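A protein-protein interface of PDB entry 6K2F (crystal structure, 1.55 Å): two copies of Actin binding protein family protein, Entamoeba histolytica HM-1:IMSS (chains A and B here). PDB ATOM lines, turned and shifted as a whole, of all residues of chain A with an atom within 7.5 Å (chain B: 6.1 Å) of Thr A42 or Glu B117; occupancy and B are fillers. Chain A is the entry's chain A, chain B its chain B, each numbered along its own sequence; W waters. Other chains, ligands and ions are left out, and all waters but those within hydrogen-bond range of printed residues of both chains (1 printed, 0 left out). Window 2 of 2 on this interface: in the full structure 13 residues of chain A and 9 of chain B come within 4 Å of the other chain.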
ATOM      1  N   GLY A  19     -16.042  17.190  -9.592  1.00  0.00           N
ATOM      2  CA  GLY A  19     -16.438  18.571  -9.918  1.00  0.00           C
ATOM      3  C   GLY A  19     -17.409  19.161  -8.909  1.00  0.00           C
ATOM      4  O   GLY A  19     -18.027  20.177  -9.236  1.00  0.00           O
ATOM      5  N   GLY A  21     -17.463  20.608  -5.825  1.00  0.00           N
ATOM      6  CA  GLY A  21     -17.096  21.654  -4.855  1.00  0.00           C
ATOM      7  C   GLY A  21     -16.269  22.679  -5.583  1.00  0.00           C
ATOM      8  O   GLY A  21     -15.898  22.410  -6.745  1.00  0.00           O
ATOM      9  N   ARG A  22     -15.938  23.782  -4.929  1.00  0.00           N
ATOM     10  CA  ARG A  22     -15.216  24.878  -5.600  1.00  0.00           C
ATOM     11  C   ARG A  22     -13.781  24.982  -5.086  1.00  0.00           C
ATOM     12  O   ARG A  22     -12.880  25.197  -5.916  1.00  0.00           O
ATOM     13  CB  ARG A  22     -15.969  26.194  -5.427  1.00  0.00           C
ATOM     14  CG  ARG A  22     -15.269  27.360  -6.111  1.00  0.00           C
ATOM     15  CD  ARG A  22     -15.118  27.210  -7.620  1.00  0.00           C
ATOM     16  NE  ARG A  22     -16.408  27.282  -8.281  1.00  0.00           N
ATOM     17  CZ  ARG A  22     -16.617  27.071  -9.567  1.00  0.00           C
ATOM     18  NH1 ARG A  22     -15.625  26.731 -10.374  1.00  0.00           N
ATOM     19  NH2 ARG A  22     -17.842  27.163 -10.053  1.00  0.00           N
ATOM     20  N   GLU A  39     -15.073  24.645   0.573  1.00  0.00           N
ATOM     21  CA  GLU A  39     -16.221  25.456   0.120  1.00  0.00           C
ATOM     22  C   GLU A  39     -16.861  24.771  -1.089  1.00  0.00           C
ATOM     23  O   GLU A  39     -16.169  24.595  -2.121  1.00  0.00           O
ATOM     24  CB  GLU A  39     -15.754  26.863  -0.239  1.00  0.00           C
ATOM     25  CG  GLU A  39     -16.839  27.732  -0.845  1.00  0.00           C
ATOM     26  CD  GLU A  39     -18.104  27.873  -0.025  1.00  0.00           C
ATOM     27  OE1 GLU A  39     -18.002  28.341   1.149  1.00  0.00           O
ATOM     28  OE2 GLU A  39     -19.193  27.534  -0.547  1.00  0.00           O
ATOM     29  N   GLN A  40     -18.143  24.428  -0.952  1.00  0.00           N
ATOM     30  CA  GLN A  40     -18.946  23.782  -2.016  1.00  0.00           C
ATOM     31  C   GLN A  40     -19.056  24.757  -3.183  1.00  0.00           C
ATOM     32  O   GLN A  40     -18.988  24.306  -4.335  1.00  0.00           O
ATOM     33  CB  GLN A  40     -20.320  23.412  -1.472  1.00  0.00           C
ATOM     34  CG  GLN A  40     -21.259  22.867  -2.531  1.00  0.00           C
ATOM     35  CD  GLN A  40     -20.725  21.584  -3.111  1.00  0.00           C
ATOM     36  OE1 GLN A  40     -20.351  20.660  -2.390  1.00  0.00           O
ATOM     37  NE2 GLN A  40     -20.710  21.518  -4.432  1.00  0.00           N
ATOM     38  N   GLY A  41     -19.263  26.037  -2.887  1.00  0.00           N
ATOM     39  CA  GLY A  41     -19.502  27.053  -3.924  1.00  0.00           C
ATOM     40  C   GLY A  41     -20.716  26.702  -4.773  1.00  0.00           C
ATOM     41  O   GLY A  41     -21.668  26.050  -4.277  1.00  0.00           O
ATOM     42  N   THR A  42     -20.697  27.141  -6.028  1.00  0.00           N
ATOM     43  CA  THR A  42     -21.848  27.121  -6.951  1.00  0.00           C
ATOM     44  C   THR A  42     -21.337  26.790  -8.359  1.00  0.00           C
ATOM     45  O   THR A  42     -20.139  26.512  -8.531  1.00  0.00           O
ATOM     46  CB  THR A  42     -22.612  28.458  -6.926  1.00  0.00           C
ATOM     47  OG1 THR A  42     -21.813  29.444  -7.570  1.00  0.00           O
ATOM     48  CG2 THR A  42     -22.966  28.918  -5.528  1.00  0.00           C
ATOM     49  N   SER A  43     -22.205  26.874  -9.342  1.00  0.00           N
ATOM     50  CA  SER A  43     -21.824  26.700 -10.757  1.00  0.00           C
ATOM     51  C   SER A  43     -21.266  28.023 -11.317  1.00  0.00           C
ATOM     52  O   SER A  43     -20.960  28.037 -12.519  1.00  0.00           O
ATOM     53  CB  SER A  43     -22.991  26.227 -11.542  1.00  0.00           C
ATOM     54  OG  SER A  43     -23.994  27.219 -11.555  1.00  0.00           O
ATOM     55  N   ASP A  44     -21.224  29.106 -10.524  1.00  0.00           N
ATOM     56  CA  ASP A  44     -20.794  30.468 -10.971  1.00  0.00           C
ATOM     57  C   ASP A  44     -19.377  30.751 -10.470  1.00  0.00           C
ATOM     58  O   ASP A  44     -19.202  31.158  -9.314  1.00  0.00           O
ATOM     59  CB  ASP A  44     -21.778  31.549 -10.508  1.00  0.00           C
ATOM     60  CG  ASP A  44     -21.531  32.940 -11.089  1.00  0.00           C
ATOM     61  OD1 ASP A  44     -20.383  33.213 -11.548  1.00  0.00           O
ATOM     62  OD2 ASP A  44     -22.495  33.739 -11.085  1.00  0.00           O
ATOM     63  N   PHE A  45     -18.387  30.511 -11.324  1.00  0.00           N
ATOM     64  CA  PHE A  45     -16.949  30.687 -11.012  1.00  0.00           C
ATOM     65  C   PHE A  45     -16.701  32.120 -10.538  1.00  0.00           C
ATOM     66  O   PHE A  45     -16.023  32.338  -9.531  1.00  0.00           O
ATOM     67  CB  PHE A  45     -16.128  30.366 -12.259  1.00  0.00           C
ATOM     68  CG  PHE A  45     -14.681  30.772 -12.186  1.00  0.00           C
ATOM     69  CD1 PHE A  45     -13.755  29.930 -11.607  1.00  0.00           C
ATOM     70  CD2 PHE A  45     -14.246  31.980 -12.702  1.00  0.00           C
ATOM     71  CE1 PHE A  45     -12.414  30.264 -11.573  1.00  0.00           C
ATOM     72  CE2 PHE A  45     -12.902  32.314 -12.658  1.00  0.00           C
ATOM     73  CZ  PHE A  45     -11.993  31.465 -12.087  1.00  0.00           C
ATOM     74  N   ASP A  46     -17.248  33.087 -11.272  1.00  0.00           N
ATOM     75  CA  ASP A  46     -16.981  34.523 -11.004  1.00  0.00           C
ATOM     76  C   ASP A  46     -17.463  34.888  -9.596  1.00  0.00           C
ATOM     77  O   ASP A  46     -16.677  35.481  -8.830  1.00  0.00           O
ATOM     78  CB  ASP A  46     -17.654  35.403 -12.053  1.00  0.00           C
ATOM     79  CG  ASP A  46     -17.021  35.308 -13.434  1.00  0.00           C
ATOM     80  OD1 ASP A  46     -15.804  35.049 -13.530  1.00  0.00           O
ATOM     81  OD2 ASP A  46     -17.752  35.484 -14.411  1.00  0.00           O
ATOM     82  N   ALA A  47     -18.710  34.543  -9.261  1.00  0.00           N
ATOM     83  CA  ALA A  47     -19.303  34.794  -7.930  1.00  0.00           C
ATOM     84  C   ALA A  47     -18.463  34.081  -6.870  1.00  0.00           C
ATOM     85  O   ALA A  47     -18.170  34.663  -5.814  1.00  0.00           O
ATOM     86  CB  ALA A  47     -20.724  34.299  -7.895  1.00  0.00           C
ATOM     87  N   ASP A  48     -18.055  32.847  -7.151  1.00  0.00           N
ATOM     88  CA  ASP A  48     -17.386  32.022  -6.125  1.00  0.00           C
ATOM     89  C   ASP A  48     -16.012  32.611  -5.776  1.00  0.00           C
ATOM     90  O   ASP A  48     -15.524  32.360  -4.655  1.00  0.00           O
ATOM     91  CB  ASP A  48     -17.268  30.557  -6.546  1.00  0.00           C
ATOM     92  CG  ASP A  48     -18.571  29.764  -6.533  1.00  0.00           C
ATOM     93  OD1 ASP A  48     -19.672  30.339  -6.232  1.00  0.00           O
ATOM     94  OD2 ASP A  48     -18.478  28.551  -6.845  1.00  0.00           O
ATOM     95  N   LEU A  51     -15.974  34.275  -2.495  1.00  0.00           N
ATOM     96  CA  LEU A  51     -16.122  33.440  -1.262  1.00  0.00           C
ATOM     97  C   LEU A  51     -14.773  33.259  -0.568  1.00  0.00           C
ATOM     98  O   LEU A  51     -14.759  33.069   0.657  1.00  0.00           O
ATOM     99  CB  LEU A  51     -16.718  32.077  -1.624  1.00  0.00           C
ATOM    100  CG  LEU A  51     -18.140  32.124  -2.167  1.00  0.00           C
ATOM    101  CD1 LEU A  51     -18.576  30.735  -2.606  1.00  0.00           C
ATOM    102  CD2 LEU A  51     -19.100  32.698  -1.129  1.00  0.00           C
ATOM    103  N   ARG A  67     -11.010  25.709  -7.984  1.00  0.00           N
ATOM    104  CA  ARG A  67     -11.339  24.973  -9.228  1.00  0.00           C
ATOM    105  C   ARG A  67     -11.871  25.942 -10.287  1.00  0.00           C
ATOM    106  O   ARG A  67     -12.763  26.729  -9.978  1.00  0.00           O
ATOM    107  CB  ARG A  67     -12.367  23.887  -8.926  1.00  0.00           C
ATOM    108  CG  ARG A  67     -12.614  22.956 -10.103  1.00  0.00           C
ATOM    109  CD  ARG A  67     -13.648  21.883  -9.815  1.00  0.00           C
ATOM    110  NE  ARG A  67     -14.901  22.449  -9.335  1.00  0.00           N
ATOM    111  CZ  ARG A  67     -15.812  23.071 -10.072  1.00  0.00           C
ATOM    112  NH1 ARG A  67     -15.636  23.228 -11.374  1.00  0.00           N
ATOM    113  NH2 ARG A  67     -16.914  23.534  -9.510  1.00  0.00           N
ATOM    114  N   GLU A  69     -13.523  26.508 -14.391  1.00  0.00           N
ATOM    115  CA  GLU A  69     -14.552  25.848 -15.238  1.00  0.00           C
ATOM    116  C   GLU A  69     -13.924  25.102 -16.416  1.00  0.00           C
ATOM    117  O   GLU A  69     -14.673  24.541 -17.222  1.00  0.00           O
ATOM    118  CB  GLU A  69     -15.530  26.898 -15.757  1.00  0.00           C
ATOM    119  CG  GLU A  69     -16.431  27.463 -14.679  1.00  0.00           C
ATOM    120  CD  GLU A  69     -17.206  26.397 -13.931  1.00  0.00           C
ATOM    121  OE1 GLU A  69     -17.911  25.603 -14.582  1.00  0.00           O
ATOM    122  OE2 GLU A  69     -17.041  26.317 -12.717  1.00  0.00           O
ATOM    123  N   LEU B  81     -35.959  27.798  -7.723  1.00  0.00           N
ATOM    124  CA  LEU B  81     -34.770  27.194  -7.094  1.00  0.00           C
ATOM    125  C   LEU B  81     -34.244  26.095  -8.012  1.00  0.00           C
ATOM    126  O   LEU B  81     -35.055  25.339  -8.576  1.00  0.00           O
ATOM    127  CB  LEU B  81     -35.137  26.595  -5.746  1.00  0.00           C
ATOM    128  CG  LEU B  81     -35.928  27.474  -4.788  1.00  0.00           C
ATOM    129  CD1 LEU B  81     -36.238  26.701  -3.516  1.00  0.00           C
ATOM    130  CD2 LEU B  81     -35.201  28.754  -4.458  1.00  0.00           C
ATOM    131  N   LEU B  82     -32.932  26.022  -8.160  1.00  0.00           N
ATOM    132  CA  LEU B  82     -32.287  24.856  -8.785  1.00  0.00           C
ATOM    133  C   LEU B  82     -31.731  24.018  -7.641  1.00  0.00           C
ATOM    134  O   LEU B  82     -30.758  24.457  -6.991  1.00  0.00           O
ATOM    135  CB  LEU B  82     -31.181  25.289  -9.737  1.00  0.00           C
ATOM    136  CG  LEU B  82     -30.405  24.135 -10.363  1.00  0.00           C
ATOM    137  CD1 LEU B  82     -31.325  23.137 -11.032  1.00  0.00           C
ATOM    138  CD2 LEU B  82     -29.403  24.703 -11.366  1.00  0.00           C
ATOM    139  N   LEU B  83     -32.370  22.902  -7.358  1.00  0.00           N
ATOM    140  CA  LEU B  83     -31.934  21.965  -6.321  1.00  0.00           C
ATOM    141  C   LEU B  83     -31.131  20.892  -7.036  1.00  0.00           C
ATOM    142  O   LEU B  83     -31.642  20.298  -8.007  1.00  0.00           O
ATOM    143  CB  LEU B  83     -33.151  21.372  -5.617  1.00  0.00           C
ATOM    144  CG  LEU B  83     -34.184  22.358  -5.065  1.00  0.00           C
ATOM    145  CD1 LEU B  83     -35.249  21.612  -4.270  1.00  0.00           C
ATOM    146  CD2 LEU B  83     -33.545  23.410  -4.181  1.00  0.00           C
ATOM    147  N   ALA B  84     -29.909  20.646  -6.597  1.00  0.00           N
ATOM    148  CA  ALA B  84     -29.060  19.617  -7.227  1.00  0.00           C
ATOM    149  C   ALA B  84     -28.718  18.621  -6.126  1.00  0.00           C
ATOM    150  O   ALA B  84     -27.956  18.979  -5.235  1.00  0.00           O
ATOM    151  CB  ALA B  84     -27.843  20.210  -7.856  1.00  0.00           C
ATOM    152  N   LYS B 102     -24.893  21.898 -14.155  1.00  0.00           N
ATOM    153  CA  LYS B 102     -25.771  22.827 -13.378  1.00  0.00           C
ATOM    154  C   LYS B 102     -26.004  24.130 -14.139  1.00  0.00           C
ATOM    155  O   LYS B 102     -27.140  24.645 -14.134  1.00  0.00           O
ATOM    156  CB  LYS B 102     -25.147  23.151 -12.018  1.00  0.00           C
ATOM    157  CG  LYS B 102     -25.374  22.134 -10.917  1.00  0.00           C
ATOM    158  CD  LYS B 102     -24.495  22.550  -9.743  1.00  0.00           C
ATOM    159  CE  LYS B 102     -24.445  21.672  -8.528  1.00  0.00           C
ATOM    160  NZ  LYS B 102     -23.443  22.265  -7.606  1.00  0.00           N
ATOM    161  N   ALA B 103     -24.954  24.694 -14.734  1.00  0.00           N
ATOM    162  CA  ALA B 103     -25.005  26.025 -15.357  1.00  0.00           C
ATOM    163  C   ALA B 103     -25.905  26.002 -16.598  1.00  0.00           C
ATOM    164  O   ALA B 103     -26.300  27.074 -17.035  1.00  0.00           O
ATOM    165  CB  ALA B 103     -23.615  26.479 -15.690  1.00  0.00           C
ATOM    166  N   ARG B 106     -29.540  27.956 -16.331  1.00  0.00           N
ATOM    167  CA  ARG B 106     -29.651  29.437 -16.441  1.00  0.00           C
ATOM    168  C   ARG B 106     -29.316  29.843 -17.873  1.00  0.00           C
ATOM    169  O   ARG B 106     -29.961  30.780 -18.374  1.00  0.00           O
ATOM    170  CB  ARG B 106     -28.852  30.186 -15.368  1.00  0.00           C
ATOM    171  CG  ARG B 106     -27.342  30.082 -15.445  1.00  0.00           C
ATOM    172  CD  ARG B 106     -26.695  30.985 -14.401  1.00  0.00           C
ATOM    173  NE  ARG B 106     -25.239  30.887 -14.435  1.00  0.00           N
ATOM    174  CZ  ARG B 106     -24.536  29.904 -13.872  1.00  0.00           C
ATOM    175  NH1 ARG B 106     -25.148  28.940 -13.210  1.00  0.00           N
ATOM    176  NH2 ARG B 106     -23.219  29.896 -13.964  1.00  0.00           N
ATOM    177  N   PHE B 114     -33.385  31.807 -11.749  1.00  0.00           N
ATOM    178  CA  PHE B 114     -33.100  31.145 -10.456  1.00  0.00           C
ATOM    179  C   PHE B 114     -32.762  32.167  -9.383  1.00  0.00           C
ATOM    180  O   PHE B 114     -31.836  32.976  -9.532  1.00  0.00           O
ATOM    181  CB  PHE B 114     -32.002  30.097 -10.599  1.00  0.00           C
ATOM    182  CG  PHE B 114     -32.417  28.990 -11.519  1.00  0.00           C
ATOM    183  CD1 PHE B 114     -33.353  28.043 -11.126  1.00  0.00           C
ATOM    184  CD2 PHE B 114     -31.986  28.977 -12.833  1.00  0.00           C
ATOM    185  CE1 PHE B 114     -33.785  27.059 -12.001  1.00  0.00           C
ATOM    186  CE2 PHE B 114     -32.413  27.985 -13.702  1.00  0.00           C
ATOM    187  CZ  PHE B 114     -33.298  27.022 -13.283  1.00  0.00           C
ATOM    188  N   LEU B 115     -33.532  32.100  -8.306  1.00  0.00           N
ATOM    189  CA  LEU B 115     -33.278  32.886  -7.085  1.00  0.00           C
ATOM    190  C   LEU B 115     -32.036  32.307  -6.423  1.00  0.00           C
ATOM    191  O   LEU B 115     -31.112  33.076  -6.091  1.00  0.00           O
ATOM    192  CB  LEU B 115     -34.501  32.788  -6.182  1.00  0.00           C
ATOM    193  CG  LEU B 115     -34.485  33.652  -4.929  1.00  0.00           C
ATOM    194  CD1 LEU B 115     -34.622  35.126  -5.269  1.00  0.00           C
ATOM    195  CD2 LEU B 115     -35.605  33.226  -3.992  1.00  0.00           C
ATOM    196  N   TYR B 116     -31.999  30.989  -6.288  1.00  0.00           N
ATOM    197  CA  TYR B 116     -30.857  30.273  -5.663  1.00  0.00           C
ATOM    198  C   TYR B 116     -30.611  28.938  -6.363  1.00  0.00           C
ATOM    199  O   TYR B 116     -31.534  28.309  -6.866  1.00  0.00           O
ATOM    200  CB  TYR B 116     -31.135  29.945  -4.200  1.00  0.00           C
ATOM    201  CG  TYR B 116     -31.449  31.121  -3.317  1.00  0.00           C
ATOM    202  CD1 TYR B 116     -30.482  32.078  -3.061  1.00  0.00           C
ATOM    203  CD2 TYR B 116     -32.686  31.245  -2.705  1.00  0.00           C
ATOM    204  CE1 TYR B 116     -30.750  33.162  -2.241  1.00  0.00           C
ATOM    205  CE2 TYR B 116     -32.959  32.315  -1.869  1.00  0.00           C
ATOM    206  CZ  TYR B 116     -32.001  33.288  -1.666  1.00  0.00           C
ATOM    207  OH  TYR B 116     -32.252  34.362  -0.861  1.00  0.00           O
ATOM    208  N   GLU B 117     -29.352  28.521  -6.311  1.00  0.00           N
ATOM    209  CA  GLU B 117     -28.882  27.184  -6.687  1.00  0.00           C
ATOM    210  C   GLU B 117     -28.447  26.520  -5.384  1.00  0.00           C
ATOM    211  O   GLU B 117     -27.623  27.125  -4.659  1.00  0.00           O
ATOM    212  CB  GLU B 117     -27.735  27.361  -7.670  1.00  0.00           C
ATOM    213  CG  GLU B 117     -27.163  26.094  -8.229  1.00  0.00           C
ATOM    214  CD  GLU B 117     -25.946  26.473  -9.058  1.00  0.00           C
ATOM    215  OE1 GLU B 117     -26.098  26.922 -10.210  1.00  0.00           O
ATOM    216  OE2 GLU B 117     -24.882  26.431  -8.488  1.00  0.00           O
ATOM    217  N   ILE B 118     -29.059  25.395  -5.055  1.00  0.00           N
ATOM    218  CA  ILE B 118     -28.850  24.678  -3.781  1.00  0.00           C
ATOM    219  C   ILE B 118     -28.297  23.293  -4.078  1.00  0.00           C
ATOM    220  O   ILE B 118     -29.029  22.431  -4.567  1.00  0.00           O
ATOM    221  CB  ILE B 118     -30.121  24.649  -2.926  1.00  0.00           C
ATOM    222  CG1 ILE B 118     -30.662  26.063  -2.701  1.00  0.00           C
ATOM    223  CG2 ILE B 118     -29.798  23.971  -1.599  1.00  0.00           C
ATOM    224  CD1 ILE B 118     -31.975  26.083  -1.938  1.00  0.00           C
ATOM    225  N   HIS B 119     -27.026  23.090  -3.758  1.00  0.00           N
ATOM    226  CA  HIS B 119     -26.368  21.775  -3.902  1.00  0.00           C
ATOM    227  C   HIS B 119     -26.520  21.014  -2.582  1.00  0.00           C
ATOM    228  O   HIS B 119     -26.240  21.587  -1.511  1.00  0.00           O
ATOM    229  CB  HIS B 119     -24.910  21.996  -4.310  1.00  0.00           C
ATOM    230  CG  HIS B 119     -24.119  20.739  -4.410  1.00  0.00           C
ATOM    231  ND1 HIS B 119     -23.743  20.188  -5.602  1.00  0.00           N
ATOM    232  CD2 HIS B 119     -23.582  19.965  -3.434  1.00  0.00           C
ATOM    233  CE1 HIS B 119     -23.030  19.093  -5.361  1.00  0.00           C
ATOM    234  NE2 HIS B 119     -22.933  18.939  -4.046  1.00  0.00           N
ATOM    235  N   PHE B 134     -30.286  26.432   4.328  1.00  0.00           N
ATOM    236  CA  PHE B 134     -29.604  27.133   3.217  1.00  0.00           C
ATOM    237  C   PHE B 134     -29.722  28.645   3.422  1.00  0.00           C
ATOM    238  O   PHE B 134     -28.708  29.388   3.295  1.00  0.00           O
ATOM    239  CB  PHE B 134     -30.171  26.717   1.870  1.00  0.00           C
ATOM    240  CG  PHE B 134     -29.667  27.598   0.763  1.00  0.00           C
ATOM    241  CD1 PHE B 134     -28.428  27.361   0.195  1.00  0.00           C
ATOM    242  CD2 PHE B 134     -30.419  28.677   0.330  1.00  0.00           C
ATOM    243  CE1 PHE B 134     -27.974  28.168  -0.836  1.00  0.00           C
ATOM    244  CE2 PHE B 134     -29.945  29.501  -0.678  1.00  0.00           C
ATOM    245  CZ  PHE B 134     -28.714  29.248  -1.241  1.00  0.00           C
HETATM  246  O   HOH W   1     -20.573  17.953  -2.852  1.00  0.00           O
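The side-chain amide nitrogen (NE2) of Gln A40 sits close to a ring nitrogen (NE2) of His B119 (3.4 Å).
OG of Ser A43 sits at hydrogen-bond distance from NH1 of Arg B106, at 2.7 Å.
OE1 of Glu B117 is in hydrogen-bond range of OG of Ser A43, at 2.5 Å.
The backbone NH of Arg A22 sits at hydrogen-bond distance from the backbone carbonyl oxygen of Gln A40, 3.2 Å away.
N of Asp A44 sits at hydrogen-bond distance from OG1 of Thr A42 (3.0 Å).
The side-chain hydroxyl (OG1) of Thr A42 is in hydrogen-bond range of the side-chain carboxylate (OD1) of Asp A48, 2.7 Å away.
OD1 of Asp A44 lies within hydrogen-bond range of N of Asp A46.
The side-chain amino group (NZ) of Lys B102 is in hydrogen-bond range of a ring nitrogen (ND1) of His B119 (2.9 Å).
NH1 of Arg B106 lies within salt-bridge range of OE1 of Glu B117 (3.7 Å).
OE2 of Glu B117 touches CB of Thr A42, at 3.4 Å.
CB of Ser A43 touches CB of Lys B102, at 3.8 Å.
Asp A44 touches Arg B106.
Thr A42 touches just one residue of chain B: Glu B117 (3.4 Å).
Printed residues of chain B within 4 Å of Ser A43: Lys B102, Arg B106 and Glu B117.
Arg A67 touches none of the printed residues of chain B.
Of the printed residues of chain A, Arg B106 touches Ser A43 and Asp A44.
Printed residues of chain A within 4 Å of Glu B117: Thr A42 and Ser A43.
The nearest residue of chain B that does not touch Thr A42 is Lys B102 (5.0 Å).
The nearest residue of chain A that does not touch Glu B117 is Asp A44 (5.0 Å).
Of the 14 printed residues of chain B, 4 touch a printed residue of chain A.
No position is printed for both chains.
Of the 6 pairs that touch across the chains among the printed residues, none has its exchanged pair printed and touching as well.
Water W1 lies within hydrogen-bond range of the side-chain amide oxygen (OE1) of Gln A40 (2.8 Å) and a ring nitrogen (NE2) of His B119 (2.8 Å).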
